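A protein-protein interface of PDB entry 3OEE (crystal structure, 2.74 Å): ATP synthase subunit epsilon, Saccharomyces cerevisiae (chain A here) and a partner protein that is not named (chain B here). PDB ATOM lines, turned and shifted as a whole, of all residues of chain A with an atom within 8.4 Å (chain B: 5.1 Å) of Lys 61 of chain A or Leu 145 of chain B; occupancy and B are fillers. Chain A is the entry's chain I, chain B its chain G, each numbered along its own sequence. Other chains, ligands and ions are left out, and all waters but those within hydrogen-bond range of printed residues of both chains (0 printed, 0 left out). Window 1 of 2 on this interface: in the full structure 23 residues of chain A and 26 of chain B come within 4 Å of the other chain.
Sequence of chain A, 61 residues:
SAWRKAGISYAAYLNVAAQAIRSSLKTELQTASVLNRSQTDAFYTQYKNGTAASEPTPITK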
ATOM      1  N   SER A   9      20.055  29.620  18.023  1.00  0.00           N
ATOM      2  CA  SER A   9      20.685  30.801  18.637  1.00  0.00           C
ATOM      3  C   SER A   9      21.779  30.383  19.638  1.00  0.00           C
ATOM      4  O   SER A   9      21.848  29.210  20.004  1.00  0.00           O
ATOM      5  CB  SER A   9      19.631  31.666  19.334  1.00  0.00           C
ATOM      6  OG  SER A   9      19.256  31.104  20.584  1.00  0.00           O
ATOM      7  N   ALA A  11      22.286  30.531  22.800  1.00  0.00           N
ATOM      8  CA  ALA A  11      21.808  29.717  23.912  1.00  0.00           C
ATOM      9  C   ALA A  11      21.487  28.297  23.424  1.00  0.00           C
ATOM     10  O   ALA A  11      22.024  27.318  23.948  1.00  0.00           O
ATOM     11  CB  ALA A  11      20.590  30.362  24.553  1.00  0.00           C
ATOM     12  N   ALA A  12      20.640  28.208  22.399  1.00  0.00           N
ATOM     13  CA  ALA A  12      20.126  26.930  21.896  1.00  0.00           C
ATOM     14  C   ALA A  12      21.193  26.088  21.208  1.00  0.00           C
ATOM     15  O   ALA A  12      21.153  24.861  21.265  1.00  0.00           O
ATOM     16  CB  ALA A  12      18.951  27.168  20.955  1.00  0.00           C
ATOM     17  N   TYR A  13      22.125  26.762  20.544  1.00  0.00           N
ATOM     18  CA  TYR A  13      23.277  26.124  19.918  1.00  0.00           C
ATOM     19  C   TYR A  13      24.081  25.392  20.985  1.00  0.00           C
ATOM     20  O   TYR A  13      24.356  24.193  20.855  1.00  0.00           O
ATOM     21  CB  TYR A  13      24.110  27.183  19.168  1.00  0.00           C
ATOM     22  CG  TYR A  13      25.608  26.945  19.072  1.00  0.00           C
ATOM     23  CD1 TYR A  13      26.495  27.691  19.851  1.00  0.00           C
ATOM     24  CD2 TYR A  13      26.137  26.002  18.185  1.00  0.00           C
ATOM     25  CE1 TYR A  13      27.868  27.492  19.768  1.00  0.00           C
ATOM     26  CE2 TYR A  13      27.512  25.794  18.093  1.00  0.00           C
ATOM     27  CZ  TYR A  13      28.370  26.543  18.888  1.00  0.00           C
ATOM     28  OH  TYR A  13      29.730  26.345  18.808  1.00  0.00           O
ATOM     29  N   LEU A  14      24.411  26.112  22.054  1.00  0.00           N
ATOM     30  CA  LEU A  14      25.159  25.549  23.168  1.00  0.00           C
ATOM     31  C   LEU A  14      24.497  24.295  23.713  1.00  0.00           C
ATOM     32  O   LEU A  14      25.177  23.323  24.058  1.00  0.00           O
ATOM     33  CB  LEU A  14      25.335  26.579  24.281  1.00  0.00           C
ATOM     34  CG  LEU A  14      26.576  27.464  24.184  1.00  0.00           C
ATOM     35  CD1 LEU A  14      26.690  28.383  25.398  1.00  0.00           C
ATOM     36  CD2 LEU A  14      27.836  26.611  24.022  1.00  0.00           C
ATOM     37  N   ASN A  15      23.165  24.326  23.765  1.00  0.00           N
ATOM     38  CA  ASN A  15      22.357  23.201  24.239  1.00  0.00           C
ATOM     39  C   ASN A  15      22.532  21.919  23.423  1.00  0.00           C
ATOM     40  O   ASN A  15      22.583  20.827  23.993  1.00  0.00           O
ATOM     41  CB  ASN A  15      20.878  23.596  24.307  1.00  0.00           C
ATOM     42  CG  ASN A  15      19.993  22.462  24.782  1.00  0.00           C
ATOM     43  OD1 ASN A  15      19.129  21.990  24.043  1.00  0.00           O
ATOM     44  ND2 ASN A  15      20.211  22.011  26.016  1.00  0.00           N
ATOM     45  N   VAL A  16      22.630  22.050  22.098  1.00  0.00           N
ATOM     46  CA  VAL A  16      22.857  20.884  21.227  1.00  0.00           C
ATOM     47  C   VAL A  16      24.248  20.277  21.480  1.00  0.00           C
ATOM     48  O   VAL A  16      24.433  19.061  21.378  1.00  0.00           O
ATOM     49  CB  VAL A  16      22.692  21.206  19.708  1.00  0.00           C
ATOM     50  CG1 VAL A  16      22.267  19.950  18.943  1.00  0.00           C
ATOM     51  CG2 VAL A  16      21.681  22.316  19.479  1.00  0.00           C
ATOM     52  N   ARG A  37      17.813  16.401  32.638  1.00  0.00           N
ATOM     53  CA  ARG A  37      18.300  17.661  32.077  1.00  0.00           C
ATOM     54  C   ARG A  37      18.284  17.667  30.538  1.00  0.00           C
ATOM     55  O   ARG A  37      18.172  18.733  29.912  1.00  0.00           O
ATOM     56  CB  ARG A  37      19.702  17.924  32.643  1.00  0.00           C
ATOM     57  CG  ARG A  37      20.568  18.959  31.935  1.00  0.00           C
ATOM     58  CD  ARG A  37      22.048  18.597  32.096  1.00  0.00           C
ATOM     59  NE  ARG A  37      22.342  18.114  33.445  1.00  0.00           N
ATOM     60  CZ  ARG A  37      23.468  17.507  33.808  1.00  0.00           C
ATOM     61  NH1 ARG A  37      24.439  17.289  32.933  1.00  0.00           N
ATOM     62  NH2 ARG A  37      23.621  17.113  35.060  1.00  0.00           N
ATOM     63  N   GLN A  39      15.869  16.471  28.726  1.00  0.00           N
ATOM     64  CA  GLN A  39      14.458  16.384  28.305  1.00  0.00           C
ATOM     65  C   GLN A  39      13.627  17.600  28.754  1.00  0.00           C
ATOM     66  O   GLN A  39      14.076  18.402  29.583  1.00  0.00           O
ATOM     67  CB  GLN A  39      13.821  15.084  28.811  1.00  0.00           C
ATOM     68  N   THR A  40      12.427  17.741  28.186  1.00  0.00           N
ATOM     69  CA  THR A  40      11.498  18.828  28.532  1.00  0.00           C
ATOM     70  C   THR A  40      10.109  18.585  27.944  1.00  0.00           C
ATOM     71  O   THR A  40       9.978  18.179  26.782  1.00  0.00           O
ATOM     72  CB  THR A  40      11.995  20.222  28.059  1.00  0.00           C
ATOM     73  N   ASP A  41       9.082  18.827  28.761  1.00  0.00           N
ATOM     74  CA  ASP A  41       7.676  18.723  28.342  1.00  0.00           C
ATOM     75  C   ASP A  41       7.035  20.119  28.310  1.00  0.00           C
ATOM     76  O   ASP A  41       5.994  20.357  28.935  1.00  0.00           O
ATOM     77  CB  ASP A  41       6.864  17.805  29.278  1.00  0.00           C
ATOM     78  CG  ASP A  41       7.682  16.659  29.860  1.00  0.00           C
ATOM     79  OD1 ASP A  41       8.253  15.859  29.084  1.00  0.00           O
ATOM     80  OD2 ASP A  41       7.731  16.552  31.108  1.00  0.00           O
ATOM     81  N   ALA A  42       7.664  21.040  27.587  1.00  0.00           N
ATOM     82  CA  ALA A  42       7.173  22.408  27.517  1.00  0.00           C
ATOM     83  C   ALA A  42       6.606  22.753  26.145  1.00  0.00           C
ATOM     84  O   ALA A  42       7.263  22.572  25.111  1.00  0.00           O
ATOM     85  CB  ALA A  42       8.265  23.388  27.910  1.00  0.00           C
ATOM     86  N   PHE A  43       5.378  23.254  26.151  1.00  0.00           N
ATOM     87  CA  PHE A  43       4.698  23.617  24.917  1.00  0.00           C
ATOM     88  C   PHE A  43       4.596  25.129  24.818  1.00  0.00           C
ATOM     89  O   PHE A  43       4.159  25.799  25.754  1.00  0.00           O
ATOM     90  CB  PHE A  43       3.317  22.942  24.831  1.00  0.00           C
ATOM     91  CG  PHE A  43       3.315  21.506  25.301  1.00  0.00           C
ATOM     92  CD1 PHE A  43       2.563  21.127  26.413  1.00  0.00           C
ATOM     93  CD2 PHE A  43       4.086  20.539  24.650  1.00  0.00           C
ATOM     94  CE1 PHE A  43       2.562  19.799  26.865  1.00  0.00           C
ATOM     95  CE2 PHE A  43       4.100  19.213  25.091  1.00  0.00           C
ATOM     96  CZ  PHE A  43       3.334  18.839  26.202  1.00  0.00           C
ATOM     97  N   TYR A  44       5.039  25.674  23.695  1.00  0.00           N
ATOM     98  CA  TYR A  44       4.918  27.104  23.493  1.00  0.00           C
ATOM     99  C   TYR A  44       3.653  27.419  22.711  1.00  0.00           C
ATOM    100  O   TYR A  44       3.323  26.743  21.729  1.00  0.00           O
ATOM    101  CB  TYR A  44       6.179  27.714  22.851  1.00  0.00           C
ATOM    102  CG  TYR A  44       6.547  27.189  21.479  1.00  0.00           C
ATOM    103  CD1 TYR A  44       7.165  25.942  21.327  1.00  0.00           C
ATOM    104  CD2 TYR A  44       6.309  27.955  20.333  1.00  0.00           C
ATOM    105  CE1 TYR A  44       7.515  25.458  20.067  1.00  0.00           C
ATOM    106  CE2 TYR A  44       6.653  27.483  19.066  1.00  0.00           C
ATOM    107  CZ  TYR A  44       7.255  26.236  18.941  1.00  0.00           C
ATOM    108  OH  TYR A  44       7.598  25.766  17.694  1.00  0.00           O
ATOM    109  N   THR A  45       2.932  28.428  23.184  1.00  0.00           N
ATOM    110  CA  THR A  45       1.712  28.866  22.529  1.00  0.00           C
ATOM    111  C   THR A  45       1.723  30.385  22.419  1.00  0.00           C
ATOM    112  O   THR A  45       1.833  31.098  23.425  1.00  0.00           O
ATOM    113  CB  THR A  45       0.437  28.381  23.276  1.00  0.00           C
ATOM    114  OG1 THR A  45       0.607  27.023  23.708  1.00  0.00           O
ATOM    115  CG2 THR A  45      -0.781  28.467  22.367  1.00  0.00           C
ATOM    116  N   PRO A  58      -0.164  24.674  19.911  1.00  0.00           N
ATOM    117  CA  PRO A  58       0.853  24.495  20.941  1.00  0.00           C
ATOM    118  C   PRO A  58       1.838  23.427  20.470  1.00  0.00           C
ATOM    119  O   PRO A  58       1.438  22.288  20.204  1.00  0.00           O
ATOM    120  CB  PRO A  58       0.052  24.031  22.162  1.00  0.00           C
ATOM    121  CG  PRO A  58      -1.193  23.419  21.613  1.00  0.00           C
ATOM    122  CD  PRO A  58      -1.423  23.970  20.228  1.00  0.00           C
ATOM    123  N   ILE A  59       3.105  23.807  20.328  1.00  0.00           N
ATOM    124  CA  ILE A  59       4.129  22.897  19.816  1.00  0.00           C
ATOM    125  C   ILE A  59       5.154  22.571  20.894  1.00  0.00           C
ATOM    126  O   ILE A  59       5.498  23.430  21.708  1.00  0.00           O
ATOM    127  CB  ILE A  59       4.840  23.489  18.581  1.00  0.00           C
ATOM    128  N   THR A  60       5.632  21.330  20.901  1.00  0.00           N
ATOM    129  CA  THR A  60       6.627  20.894  21.879  1.00  0.00           C
ATOM    130  C   THR A  60       8.006  21.500  21.567  1.00  0.00           C
ATOM    131  O   THR A  60       8.707  21.026  20.668  1.00  0.00           O
ATOM    132  CB  THR A  60       6.716  19.352  21.942  1.00  0.00           C
ATOM    133  N   LYS A  61       8.383  22.551  22.299  1.00  0.00           N
ATOM    134  CA  LYS A  61       9.657  23.251  22.070  1.00  0.00           C
ATOM    135  C   LYS A  61      10.864  22.319  22.200  1.00  0.00           C
ATOM    136  O   LYS A  61      11.482  21.936  21.204  1.00  0.00           O
ATOM    137  CB  LYS A  61       9.803  24.437  23.030  1.00  0.00           C
ATOM    138  N   PHE B 140      18.792  23.775  32.055  1.00  0.00           N
ATOM    139  CA  PHE B 140      19.262  24.787  31.107  1.00  0.00           C
ATOM    140  C   PHE B 140      18.538  24.673  29.780  1.00  0.00           C
ATOM    141  O   PHE B 140      18.253  25.686  29.143  1.00  0.00           O
ATOM    142  CB  PHE B 140      20.776  24.709  30.891  1.00  0.00           C
ATOM    143  CG  PHE B 140      21.313  25.748  29.936  1.00  0.00           C
ATOM    144  CD1 PHE B 140      21.442  25.467  28.575  1.00  0.00           C
ATOM    145  CD2 PHE B 140      21.693  27.011  30.396  1.00  0.00           C
ATOM    146  CE1 PHE B 140      21.934  26.423  27.694  1.00  0.00           C
ATOM    147  CE2 PHE B 140      22.190  27.969  29.521  1.00  0.00           C
ATOM    148  CZ  PHE B 140      22.307  27.679  28.172  1.00  0.00           C
ATOM    149  N   GLN B 141      18.243  23.442  29.369  1.00  0.00           N
ATOM    150  CA  GLN B 141      17.519  23.214  28.126  1.00  0.00           C
ATOM    151  C   GLN B 141      16.249  24.055  28.106  1.00  0.00           C
ATOM    152  O   GLN B 141      16.027  24.823  27.167  1.00  0.00           O
ATOM    153  CB  GLN B 141      17.194  21.737  27.954  1.00  0.00           C
ATOM    154  CG  GLN B 141      16.818  21.346  26.539  1.00  0.00           C
ATOM    155  CD  GLN B 141      17.124  19.886  26.247  1.00  0.00           C
ATOM    156  OE1 GLN B 141      16.752  18.991  27.017  1.00  0.00           O
ATOM    157  NE2 GLN B 141      17.810  19.636  25.133  1.00  0.00           N
ATOM    158  N   GLU B 142      15.438  23.919  29.156  1.00  0.00           N
ATOM    159  CA  GLU B 142      14.225  24.720  29.313  1.00  0.00           C
ATOM    160  C   GLU B 142      14.577  26.194  29.187  1.00  0.00           C
ATOM    161  O   GLU B 142      14.125  26.883  28.272  1.00  0.00           O
ATOM    162  CB  GLU B 142      13.554  24.457  30.669  1.00  0.00           C
ATOM    163  CG  GLU B 142      12.952  23.058  30.827  1.00  0.00           C
ATOM    164  CD  GLU B 142      12.052  22.915  32.061  1.00  0.00           C
ATOM    165  OE1 GLU B 142      11.932  23.886  32.847  1.00  0.00           O
ATOM    166  OE2 GLU B 142      11.460  21.824  32.241  1.00  0.00           O
ATOM    167  N   SER B 143      15.418  26.653  30.104  1.00  0.00           N
ATOM    168  CA  SER B 143      15.874  28.027  30.135  1.00  0.00           C
ATOM    169  C   SER B 143      16.349  28.515  28.773  1.00  0.00           C
ATOM    170  O   SER B 143      16.128  29.676  28.418  1.00  0.00           O
ATOM    171  CB  SER B 143      17.001  28.164  31.151  1.00  0.00           C
ATOM    172  OG  SER B 143      17.245  29.528  31.429  1.00  0.00           O
ATOM    173  N   ALA B 144      16.993  27.625  28.017  1.00  0.00           N
ATOM    174  CA  ALA B 144      17.554  27.966  26.709  1.00  0.00           C
ATOM    175  C   ALA B 144      16.486  28.063  25.613  1.00  0.00           C
ATOM    176  O   ALA B 144      16.368  29.097  24.945  1.00  0.00           O
ATOM    177  CB  ALA B 144      18.653  26.979  26.316  1.00  0.00           C
ATOM    178  N   LEU B 145      15.710  26.990  25.435  1.00  0.00           N
ATOM    179  CA  LEU B 145      14.709  26.933  24.366  1.00  0.00           C
ATOM    180  C   LEU B 145      13.620  27.987  24.536  1.00  0.00           C
ATOM    181  O   LEU B 145      13.102  28.507  23.550  1.00  0.00           O
ATOM    182  CB  LEU B 145      14.108  25.532  24.234  1.00  0.00           C
ATOM    183  CG  LEU B 145      14.818  24.534  23.311  1.00  0.00           C
ATOM    184  CD1 LEU B 145      16.179  24.116  23.849  1.00  0.00           C
ATOM    185  CD2 LEU B 145      13.956  23.307  23.085  1.00  0.00           C
ATOM    186  N   ILE B 146      13.283  28.305  25.786  1.00  0.00           N
ATOM    187  CA  ILE B 146      12.416  29.445  26.082  1.00  0.00           C
ATOM    188  C   ILE B 146      13.101  30.743  25.634  1.00  0.00           C
ATOM    189  O   ILE B 146      12.470  31.608  25.020  1.00  0.00           O
ATOM    190  CB  ILE B 146      12.027  29.512  27.580  1.00  0.00           C
ATOM    191  CG1 ILE B 146      11.139  28.315  27.957  1.00  0.00           C
ATOM    192  CG2 ILE B 146      11.319  30.826  27.887  1.00  0.00           C
ATOM    193  CD1 ILE B 146      10.815  28.185  29.440  1.00  0.00           C
ATOM    194  N   ALA B 147      14.396  30.865  25.923  1.00  0.00           N
ATOM    195  CA  ALA B 147      15.164  32.012  25.449  1.00  0.00           C
ATOM    196  C   ALA B 147      15.125  32.050  23.930  1.00  0.00           C
ATOM    197  O   ALA B 147      14.852  33.091  23.341  1.00  0.00           O
ATOM    198  CB  ALA B 147      16.602  31.957  25.956  1.00  0.00           C
ATOM    199  N   ASP B 148      15.368  30.897  23.309  1.00  0.00           N
ATOM    200  CA  ASP B 148      15.406  30.774  21.853  1.00  0.00           C
ATOM    201  C   ASP B 148      14.152  31.360  21.198  1.00  0.00           C
ATOM    202  O   ASP B 148      14.236  32.073  20.193  1.00  0.00           O
ATOM    203  CB  ASP B 148      15.583  29.303  21.442  1.00  0.00           C
ATOM    204  CG  ASP B 148      16.122  29.149  20.024  1.00  0.00           C
ATOM    205  OD1 ASP B 148      17.320  29.422  19.807  1.00  0.00           O
ATOM    206  OD2 ASP B 148      15.355  28.741  19.127  1.00  0.00           O
ATOM    207  N   LYS B 149      12.998  31.075  21.787  1.00  0.00           N
ATOM    208  CA  LYS B 149      11.727  31.498  21.220  1.00  0.00           C
ATOM    209  C   LYS B 149      11.429  32.966  21.520  1.00  0.00           C
ATOM    210  O   LYS B 149      10.748  33.642  20.741  1.00  0.00           O
ATOM    211  CB  LYS B 149      10.596  30.582  21.697  1.00  0.00           C
ATOM    212  CG  LYS B 149      10.789  29.101  21.339  1.00  0.00           C
ATOM    213  CD  LYS B 149      10.481  28.801  19.869  1.00  0.00           C
ATOM    214  CE  LYS B 149      10.789  27.347  19.513  1.00  0.00           C
ATOM    215  NZ  LYS B 149      12.257  27.066  19.509  1.00  0.00           N
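O of Arg 37 of chain A lies close to OE1 of Gln 141 of chain B (3.2 Å). The side-chain amide oxygen of Gln 141 of chain B is in hydrogen-bond range of the backbone NH of Gln 39 of chain A (3.2 Å). The side-chain amide oxygen (OD1) of Asn 15 of chain A sits at hydrogen-bond distance from the side-chain amide nitrogen (NE2) of Gln 141 of chain B (2.9 Å). OD1 of Asp 148 of chain B lies within hydrogen-bond range of OG of Ser 9 of chain A (2.7 Å).
Of the 19 printed residues of chain A, 8 touch a printed residue of chain B. Hydrophobic or aromatic side chains of chain A that line the printed part of chain B: Ala 12 and Tyr 44. Among the printed residues, 9 pairs touch across the chains.
CE1 of Phe 140 of chain B touches O of Ala 11 of chain A, 3.9 Å away. Ala 12 of chain A touches Asp 148 of chain B (CB to OD1, 3.0 Å). OD1 of Asn 15 of chain A touches CD1 of Leu 145 of chain B, at 3.6 Å. Lys 149 of chain B touches Tyr 44 of chain A. Leu 145 of chain B touches Lys 61 of chain A (CD2 to C, 3.4 Å).
The backbone NH (N) of Lys 61 of chain A is in hydrogen-bond range of the backbone carbonyl oxygen (O) of Ala 42 of chain A, 3.0 Å away. The backbone NH (N) of Tyr 44 of chain A is in hydrogen-bond range of the backbone carbonyl oxygen (O) of Ile 59 of chain A (3.0 Å). OD2 of Asp 148 of chain B lies within salt-bridge range of NZ of Lys 149 of chain B (3.5 Å).
Lys 61 of chain A touches one residue of chain B. Leu 145 of chain B touches two residues of chain A. Of the printed residues of chain A, Gln 141 of chain B touches Asn 15, Arg 37 and Gln 39. Of the printed residues of chain A, Asp 148 of chain B touches Ser 9 (2.7 Å) and Ala 12 (3.0 Å). Printed residues of chain B within 4 Å of Asn 15 of chain A: Gln 141 and Leu 145. Of the printed residues of chain A, Lys 149 of chain B touches Tyr 44. Printed residues of chain B within 4 Å of Ala 12 of chain A: Asp 148. Thr 60 of chain A touches none of the printed residues of chain B. The nearest printed residue of chain B that does not touch Ala 11 of chain A is Ala 144 of chain B (4.1 Å).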
